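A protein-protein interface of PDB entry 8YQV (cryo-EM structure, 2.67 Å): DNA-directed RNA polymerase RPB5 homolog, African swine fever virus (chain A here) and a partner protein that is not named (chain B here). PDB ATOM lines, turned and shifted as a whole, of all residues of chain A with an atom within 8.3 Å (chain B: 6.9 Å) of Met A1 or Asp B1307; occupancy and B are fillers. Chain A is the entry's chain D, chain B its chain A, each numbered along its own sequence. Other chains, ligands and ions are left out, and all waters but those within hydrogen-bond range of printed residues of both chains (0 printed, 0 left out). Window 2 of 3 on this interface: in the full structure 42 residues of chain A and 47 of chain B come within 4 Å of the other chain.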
ATOM      1  N   MET A   1     -16.415   4.999 -15.653  1.00  0.00           N
ATOM      2  CA  MET A   1     -17.006   5.097 -16.982  1.00  0.00           C
ATOM      3  C   MET A   1     -18.252   4.221 -17.004  1.00  0.00           C
ATOM      4  O   MET A   1     -18.823   3.947 -18.055  1.00  0.00           O
ATOM      5  CB  MET A   1     -15.992   4.674 -18.054  1.00  0.00           C
ATOM      6  CG  MET A   1     -16.419   4.903 -19.500  1.00  0.00           C
ATOM      7  SD  MET A   1     -15.108   5.619 -20.511  1.00  0.00           S
ATOM      8  CE  MET A   1     -15.524   7.360 -20.446  1.00  0.00           C
ATOM      9  N   ALA A   2     -18.685   3.816 -15.807  1.00  0.00           N
ATOM     10  CA  ALA A   2     -19.776   2.854 -15.692  1.00  0.00           C
ATOM     11  C   ALA A   2     -21.063   3.379 -16.314  1.00  0.00           C
ATOM     12  O   ALA A   2     -21.792   2.623 -16.963  1.00  0.00           O
ATOM     13  CB  ALA A   2     -20.004   2.492 -14.228  1.00  0.00           C
ATOM     14  N   MET A   3     -21.367   4.662 -16.128  1.00  0.00           N
ATOM     15  CA  MET A   3     -22.641   5.186 -16.607  1.00  0.00           C
ATOM     16  C   MET A   3     -22.682   5.316 -18.124  1.00  0.00           C
ATOM     17  O   MET A   3     -23.723   5.052 -18.736  1.00  0.00           O
ATOM     18  CB  MET A   3     -22.932   6.534 -15.949  1.00  0.00           C
ATOM     19  CG  MET A   3     -24.410   6.819 -15.730  1.00  0.00           C
ATOM     20  SD  MET A   3     -25.330   5.566 -14.798  1.00  0.00           S
ATOM     21  CE  MET A   3     -24.166   5.103 -13.511  1.00  0.00           C
ATOM     22  N   GLN A   4     -21.577   5.722 -18.749  1.00  0.00           N
ATOM     23  CA  GLN A   4     -21.551   5.792 -20.205  1.00  0.00           C
ATOM     24  C   GLN A   4     -21.684   4.406 -20.820  1.00  0.00           C
ATOM     25  O   GLN A   4     -22.356   4.239 -21.844  1.00  0.00           O
ATOM     26  CB  GLN A   4     -20.262   6.464 -20.679  1.00  0.00           C
ATOM     27  CG  GLN A   4     -20.106   6.771 -22.190  1.00  0.00           C
ATOM     28  CD  GLN A   4     -21.359   7.271 -22.927  1.00  0.00           C
ATOM     29  OE1 GLN A   4     -22.452   6.714 -22.824  1.00  0.00           O
ATOM     30  NE2 GLN A   4     -21.179   8.338 -23.697  1.00  0.00           N
ATOM     31  N   LYS A   5     -21.051   3.400 -20.214  1.00  0.00           N
ATOM     32  CA  LYS A   5     -21.211   2.031 -20.687  1.00  0.00           C
ATOM     33  C   LYS A   5     -22.633   1.525 -20.475  1.00  0.00           C
ATOM     34  O   LYS A   5     -23.188   0.848 -21.349  1.00  0.00           O
ATOM     35  CB  LYS A   5     -20.200   1.120 -19.995  1.00  0.00           C
ATOM     36  CG  LYS A   5     -18.766   1.494 -20.285  1.00  0.00           C
ATOM     37  CD  LYS A   5     -18.537   1.499 -21.781  1.00  0.00           C
ATOM     38  CE  LYS A   5     -17.150   1.980 -22.138  1.00  0.00           C
ATOM     39  NZ  LYS A   5     -16.990   2.102 -23.608  1.00  0.00           N
ATOM     40  N   LEU A   6     -23.231   1.848 -19.328  1.00  0.00           N
ATOM     41  CA  LEU A   6     -24.609   1.452 -19.073  1.00  0.00           C
ATOM     42  C   LEU A   6     -25.549   2.040 -20.108  1.00  0.00           C
ATOM     43  O   LEU A   6     -26.390   1.328 -20.656  1.00  0.00           O
ATOM     44  CB  LEU A   6     -25.040   1.889 -17.678  1.00  0.00           C
ATOM     45  CG  LEU A   6     -24.778   0.960 -16.500  1.00  0.00           C
ATOM     46  CD1 LEU A   6     -25.077   1.684 -15.208  1.00  0.00           C
ATOM     47  CD2 LEU A   6     -25.631  -0.274 -16.616  1.00  0.00           C
ATOM     48  N   PHE A   7     -25.408   3.329 -20.412  1.00  0.00           N
ATOM     49  CA  PHE A   7     -26.375   3.976 -21.291  1.00  0.00           C
ATOM     50  C   PHE A   7     -26.432   3.342 -22.676  1.00  0.00           C
ATOM     51  O   PHE A   7     -27.436   3.505 -23.376  1.00  0.00           O
ATOM     52  CB  PHE A   7     -26.066   5.464 -21.418  1.00  0.00           C
ATOM     53  CG  PHE A   7     -27.072   6.217 -22.231  1.00  0.00           C
ATOM     54  CD1 PHE A   7     -28.317   6.515 -21.711  1.00  0.00           C
ATOM     55  CD2 PHE A   7     -26.781   6.605 -23.521  1.00  0.00           C
ATOM     56  CE1 PHE A   7     -29.243   7.201 -22.457  1.00  0.00           C
ATOM     57  CE2 PHE A   7     -27.705   7.289 -24.271  1.00  0.00           C
ATOM     58  CZ  PHE A   7     -28.938   7.585 -23.738  1.00  0.00           C
ATOM     59  N   THR A   8     -25.391   2.625 -23.090  1.00  0.00           N
ATOM     60  CA  THR A   8     -25.424   1.929 -24.369  1.00  0.00           C
ATOM     61  C   THR A   8     -25.819   0.467 -24.198  1.00  0.00           C
ATOM     62  O   THR A   8     -26.672  -0.054 -24.932  1.00  0.00           O
ATOM     63  CB  THR A   8     -24.059   2.025 -25.058  1.00  0.00           C
ATOM     64  OG1 THR A   8     -23.029   1.682 -24.125  1.00  0.00           O
ATOM     65  CG2 THR A   8     -23.814   3.431 -25.567  1.00  0.00           C
ATOM     66  N   TYR A   9     -25.224  -0.206 -23.223  1.00  0.00           N
ATOM     67  CA  TYR A   9     -25.414  -1.639 -23.137  1.00  0.00           C
ATOM     68  C   TYR A   9     -26.697  -2.040 -22.427  1.00  0.00           C
ATOM     69  O   TYR A   9     -27.135  -3.173 -22.601  1.00  0.00           O
ATOM     70  CB  TYR A   9     -24.203  -2.287 -22.474  1.00  0.00           C
ATOM     71  CG  TYR A   9     -22.940  -2.080 -23.274  1.00  0.00           C
ATOM     72  CD1 TYR A   9     -22.872  -2.462 -24.602  1.00  0.00           C
ATOM     73  CD2 TYR A   9     -21.817  -1.508 -22.705  1.00  0.00           C
ATOM     74  CE1 TYR A   9     -21.728  -2.274 -25.340  1.00  0.00           C
ATOM     75  CE2 TYR A   9     -20.669  -1.322 -23.430  1.00  0.00           C
ATOM     76  CZ  TYR A   9     -20.629  -1.705 -24.748  1.00  0.00           C
ATOM     77  OH  TYR A   9     -19.478  -1.518 -25.475  1.00  0.00           O
ATOM     78  N   TYR A  28     -27.629  11.479 -23.672  1.00  0.00           N
ATOM     79  CA  TYR A  28     -26.861  10.937 -22.561  1.00  0.00           C
ATOM     80  C   TYR A  28     -26.792  11.903 -21.390  1.00  0.00           C
ATOM     81  O   TYR A  28     -26.950  11.487 -20.238  1.00  0.00           O
ATOM     82  CB  TYR A  28     -25.451  10.571 -23.020  1.00  0.00           C
ATOM     83  CG  TYR A  28     -24.511  10.255 -21.880  1.00  0.00           C
ATOM     84  CD1 TYR A  28     -24.749   9.184 -21.035  1.00  0.00           C
ATOM     85  CD2 TYR A  28     -23.388  11.030 -21.652  1.00  0.00           C
ATOM     86  CE1 TYR A  28     -23.894   8.893 -19.991  1.00  0.00           C
ATOM     87  CE2 TYR A  28     -22.529  10.749 -20.614  1.00  0.00           C
ATOM     88  CZ  TYR A  28     -22.783   9.681 -19.785  1.00  0.00           C
ATOM     89  OH  TYR A  28     -21.924   9.406 -18.748  1.00  0.00           O
ATOM     90  N   TYR A 123     -23.303  -3.535 -11.536  1.00  0.00           N
ATOM     91  CA  TYR A 123     -23.099  -2.728 -12.734  1.00  0.00           C
ATOM     92  C   TYR A 123     -22.473  -3.538 -13.858  1.00  0.00           C
ATOM     93  O   TYR A 123     -22.848  -3.376 -15.025  1.00  0.00           O
ATOM     94  CB  TYR A 123     -22.220  -1.518 -12.421  1.00  0.00           C
ATOM     95  CG  TYR A 123     -22.952  -0.330 -11.843  1.00  0.00           C
ATOM     96  CD1 TYR A 123     -24.237  -0.016 -12.251  1.00  0.00           C
ATOM     97  CD2 TYR A 123     -22.338   0.503 -10.922  1.00  0.00           C
ATOM     98  CE1 TYR A 123     -24.899   1.070 -11.733  1.00  0.00           C
ATOM     99  CE2 TYR A 123     -22.993   1.594 -10.407  1.00  0.00           C
ATOM    100  CZ  TYR A 123     -24.271   1.872 -10.815  1.00  0.00           C
ATOM    101  OH  TYR A 123     -24.929   2.958 -10.299  1.00  0.00           O
ATOM    102  N   CYS A 127     -22.412  -3.465 -18.449  1.00  0.00           N
ATOM    103  CA  CYS A 127     -21.409  -2.555 -18.979  1.00  0.00           C
ATOM    104  C   CYS A 127     -20.684  -3.132 -20.181  1.00  0.00           C
ATOM    105  O   CYS A 127     -19.681  -2.563 -20.620  1.00  0.00           O
ATOM    106  CB  CYS A 127     -20.406  -2.177 -17.893  1.00  0.00           C
ATOM    107  SG  CYS A 127     -21.086  -1.099 -16.625  1.00  0.00           S
ATOM    108  N   LEU B1098      -5.354  -4.270 -27.669  1.00  0.00           N
ATOM    109  CA  LEU B1098      -5.536  -2.873 -28.024  1.00  0.00           C
ATOM    110  C   LEU B1098      -6.836  -2.697 -28.800  1.00  0.00           C
ATOM    111  O   LEU B1098      -7.388  -3.639 -29.367  1.00  0.00           O
ATOM    112  CB  LEU B1098      -4.343  -2.354 -28.829  1.00  0.00           C
ATOM    113  CG  LEU B1098      -3.025  -2.263 -28.055  1.00  0.00           C
ATOM    114  CD1 LEU B1098      -1.921  -1.733 -28.947  1.00  0.00           C
ATOM    115  CD2 LEU B1098      -3.167  -1.415 -26.804  1.00  0.00           C
ATOM    116  N   LYS B1099      -7.312  -1.455 -28.827  1.00  0.00           N
ATOM    117  CA  LYS B1099      -8.655  -1.154 -29.298  1.00  0.00           C
ATOM    118  C   LYS B1099      -8.847  -1.392 -30.787  1.00  0.00           C
ATOM    119  O   LYS B1099      -9.990  -1.375 -31.252  1.00  0.00           O
ATOM    120  CB  LYS B1099      -8.992   0.300 -28.980  1.00  0.00           C
ATOM    121  CG  LYS B1099      -7.946   1.283 -29.476  1.00  0.00           C
ATOM    122  CD  LYS B1099      -8.552   2.300 -30.427  1.00  0.00           C
ATOM    123  CE  LYS B1099      -7.544   3.365 -30.816  1.00  0.00           C
ATOM    124  NZ  LYS B1099      -8.199   4.545 -31.439  1.00  0.00           N
ATOM    125  N   TYR B1109       2.698   3.409 -29.468  1.00  0.00           N
ATOM    126  CA  TYR B1109       1.306   3.606 -29.087  1.00  0.00           C
ATOM    127  C   TYR B1109       0.916   2.681 -27.943  1.00  0.00           C
ATOM    128  O   TYR B1109       0.166   3.079 -27.044  1.00  0.00           O
ATOM    129  CB  TYR B1109       0.399   3.385 -30.294  1.00  0.00           C
ATOM    130  CG  TYR B1109      -1.049   3.724 -30.040  1.00  0.00           C
ATOM    131  CD1 TYR B1109      -2.057   2.822 -30.341  1.00  0.00           C
ATOM    132  CD2 TYR B1109      -1.407   4.951 -29.512  1.00  0.00           C
ATOM    133  CE1 TYR B1109      -3.380   3.132 -30.112  1.00  0.00           C
ATOM    134  CE2 TYR B1109      -2.727   5.270 -29.283  1.00  0.00           C
ATOM    135  CZ  TYR B1109      -3.708   4.359 -29.585  1.00  0.00           C
ATOM    136  OH  TYR B1109      -5.025   4.676 -29.353  1.00  0.00           O
ATOM    137  N   PHE B1301     -13.536  -5.826 -14.859  1.00  0.00           N
ATOM    138  CA  PHE B1301     -14.516  -4.758 -14.994  1.00  0.00           C
ATOM    139  C   PHE B1301     -13.849  -3.401 -15.162  1.00  0.00           C
ATOM    140  O   PHE B1301     -14.378  -2.539 -15.870  1.00  0.00           O
ATOM    141  CB  PHE B1301     -15.451  -4.746 -13.790  1.00  0.00           C
ATOM    142  CG  PHE B1301     -16.490  -3.670 -13.843  1.00  0.00           C
ATOM    143  CD1 PHE B1301     -17.267  -3.499 -14.970  1.00  0.00           C
ATOM    144  CD2 PHE B1301     -16.709  -2.848 -12.758  1.00  0.00           C
ATOM    145  CE1 PHE B1301     -18.228  -2.518 -15.020  1.00  0.00           C
ATOM    146  CE2 PHE B1301     -17.669  -1.870 -12.803  1.00  0.00           C
ATOM    147  CZ  PHE B1301     -18.432  -1.706 -13.933  1.00  0.00           C
ATOM    148  N   ALA B1303     -11.096  -2.879 -16.822  1.00  0.00           N
ATOM    149  CA  ALA B1303     -10.634  -2.814 -18.199  1.00  0.00           C
ATOM    150  C   ALA B1303     -11.757  -2.593 -19.203  1.00  0.00           C
ATOM    151  O   ALA B1303     -11.493  -2.076 -20.292  1.00  0.00           O
ATOM    152  CB  ALA B1303      -9.871  -4.087 -18.560  1.00  0.00           C
ATOM    153  N   MET B1304     -12.996  -2.969 -18.879  1.00  0.00           N
ATOM    154  CA  MET B1304     -14.109  -2.667 -19.769  1.00  0.00           C
ATOM    155  C   MET B1304     -14.521  -1.205 -19.709  1.00  0.00           C
ATOM    156  O   MET B1304     -15.016  -0.674 -20.708  1.00  0.00           O
ATOM    157  CB  MET B1304     -15.325  -3.535 -19.447  1.00  0.00           C
ATOM    158  CG  MET B1304     -15.005  -4.874 -18.836  1.00  0.00           C
ATOM    159  SD  MET B1304     -16.224  -6.123 -19.256  1.00  0.00           S
ATOM    160  CE  MET B1304     -17.370  -5.905 -17.904  1.00  0.00           C
ATOM    161  N   LEU B1305     -14.334  -0.549 -18.569  1.00  0.00           N
ATOM    162  CA  LEU B1305     -14.608   0.883 -18.443  1.00  0.00           C
ATOM    163  C   LEU B1305     -13.453   1.708 -18.997  1.00  0.00           C
ATOM    164  O   LEU B1305     -12.913   2.590 -18.335  1.00  0.00           O
ATOM    165  CB  LEU B1305     -14.880   1.231 -16.987  1.00  0.00           C
ATOM    166  CG  LEU B1305     -15.915   0.373 -16.270  1.00  0.00           C
ATOM    167  CD1 LEU B1305     -16.100   0.854 -14.849  1.00  0.00           C
ATOM    168  CD2 LEU B1305     -17.221   0.413 -17.022  1.00  0.00           C
ATOM    169  N   ASP B1306     -13.068   1.413 -20.236  1.00  0.00           N
ATOM    170  CA  ASP B1306     -11.853   1.961 -20.821  1.00  0.00           C
ATOM    171  C   ASP B1306     -11.859   1.747 -22.326  1.00  0.00           C
ATOM    172  O   ASP B1306     -11.990   0.612 -22.795  1.00  0.00           O
ATOM    173  CB  ASP B1306     -10.626   1.310 -20.183  1.00  0.00           C
ATOM    174  CG  ASP B1306      -9.343   2.004 -20.550  1.00  0.00           C
ATOM    175  OD1 ASP B1306      -9.397   3.011 -21.283  1.00  0.00           O
ATOM    176  OD2 ASP B1306      -8.276   1.540 -20.100  1.00  0.00           O
ATOM    177  N   ASP B1307     -11.715   2.827 -23.091  1.00  0.00           N
ATOM    178  CA  ASP B1307     -11.854   2.785 -24.539  1.00  0.00           C
ATOM    179  C   ASP B1307     -10.559   2.448 -25.260  1.00  0.00           C
ATOM    180  O   ASP B1307     -10.586   2.198 -26.467  1.00  0.00           O
ATOM    181  CB  ASP B1307     -12.396   4.122 -25.047  1.00  0.00           C
ATOM    182  CG  ASP B1307     -13.683   4.524 -24.358  1.00  0.00           C
ATOM    183  OD1 ASP B1307     -14.491   5.247 -24.977  1.00  0.00           O
ATOM    184  OD2 ASP B1307     -13.889   4.111 -23.198  1.00  0.00           O
ATOM    185  N   ASN B1308      -9.434   2.425 -24.558  1.00  0.00           N
ATOM    186  CA  ASN B1308      -8.163   2.071 -25.169  1.00  0.00           C
ATOM    187  C   ASN B1308      -7.934   0.569 -25.222  1.00  0.00           C
ATOM    188  O   ASN B1308      -6.969   0.123 -25.852  1.00  0.00           O
ATOM    189  CB  ASN B1308      -7.016   2.739 -24.410  1.00  0.00           C
ATOM    190  CG  ASN B1308      -7.119   4.248 -24.416  1.00  0.00           C
ATOM    191  OD1 ASN B1308      -7.278   4.875 -23.371  1.00  0.00           O
ATOM    192  ND2 ASN B1308      -7.032   4.842 -25.597  1.00  0.00           N
ATOM    193  N   ILE B1309      -8.801  -0.213 -24.590  1.00  0.00           N
ATOM    194  CA  ILE B1309      -8.663  -1.658 -24.485  1.00  0.00           C
ATOM    195  C   ILE B1309      -9.866  -2.304 -25.153  1.00  0.00           C
ATOM    196  O   ILE B1309     -11.004  -1.863 -24.956  1.00  0.00           O
ATOM    197  CB  ILE B1309      -8.550  -2.087 -23.010  1.00  0.00           C
ATOM    198  CG1 ILE B1309      -7.167  -1.749 -22.461  1.00  0.00           C
ATOM    199  CG2 ILE B1309      -8.828  -3.561 -22.855  1.00  0.00           C
ATOM    200  CD1 ILE B1309      -6.055  -1.874 -23.479  1.00  0.00           C
ATOM    201  N   ASP B1310      -9.619  -3.332 -25.953  1.00  0.00           N
ATOM    202  CA  ASP B1310     -10.714  -4.077 -26.563  1.00  0.00           C
ATOM    203  C   ASP B1310     -11.438  -4.854 -25.474  1.00  0.00           C
ATOM    204  O   ASP B1310     -10.818  -5.698 -24.816  1.00  0.00           O
ATOM    205  CB  ASP B1310     -10.188  -5.017 -27.638  1.00  0.00           C
ATOM    206  CG  ASP B1310     -11.284  -5.571 -28.517  1.00  0.00           C
ATOM    207  OD1 ASP B1310     -11.942  -4.776 -29.215  1.00  0.00           O
ATOM    208  OD2 ASP B1310     -11.476  -6.800 -28.536  1.00  0.00           O
ATOM    209  N   PRO B1311     -12.731  -4.607 -25.245  1.00  0.00           N
ATOM    210  CA  PRO B1311     -13.406  -5.201 -24.085  1.00  0.00           C
ATOM    211  C   PRO B1311     -13.841  -6.639 -24.289  1.00  0.00           C
ATOM    212  O   PRO B1311     -14.204  -7.303 -23.309  1.00  0.00           O
ATOM    213  CB  PRO B1311     -14.620  -4.289 -23.902  1.00  0.00           C
ATOM    214  CG  PRO B1311     -14.939  -3.853 -25.285  1.00  0.00           C
ATOM    215  CD  PRO B1311     -13.632  -3.735 -26.016  1.00  0.00           C
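The side-chain amino group of Lys A5 lies within salt-bridge range of the side-chain carboxylate of Asp B1307 (3.7 Å).
The side-chain carboxylate of Asp B1307 sits close to the side-chain sulfur of Met A1 (3.3 Å).
The side-chain hydroxyl (OG1) of Thr A8 lies within hydrogen-bond range of the backbone carbonyl oxygen (O) of Lys A5, 2.9 Å away.
The backbone carbonyl oxygen (O) of Tyr A123 is in hydrogen-bond range of the side-chain sulfur (SG) of Cys A127, at 3.3 Å.
Leu B1305 touches Met A1 (O to CB, 3.7 Å).
Leu B1305 touches Ala A2 (CD2 to CA, 3.8 Å).
Met B1304 touches Lys A5.
Leu B1305 touches Lys A5 (CD2 to CG, 3.8 Å).
Cys A127 touches Phe B1301.
Met A1 touches just these residues of chain B: Leu B1305 and Asp B1307.
Asp B1307 touches just these residues of chain A: Met A1 and Lys A5.
Printed residues of chain A within 4 Å of Met B1304: Lys A5 (3.7 Å).
Printed residues of chain A within 4 Å of Phe B1301: Cys A127.
Of the printed residues of chain A, Leu B1305 touches Met A1, Ala A2 and Lys A5.
Printed residues of chain B within 4 Å of Cys A127: Phe B1301.
Printed residues of chain B within 4 Å of Ala A2: Leu B1305 (3.8 Å).
The nearest printed residue of chain B that does not touch Ala A2 is Phe B1301 (4.5 Å).
Printed residues of chain A that touch a printed residue of chain B: Met A1, Ala A2, Lys A5 and Cys A127.
Printed residues of chain B that touch a printed residue of chain A: Phe B1301, Met B1304, Leu B1305 and Asp B1307.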
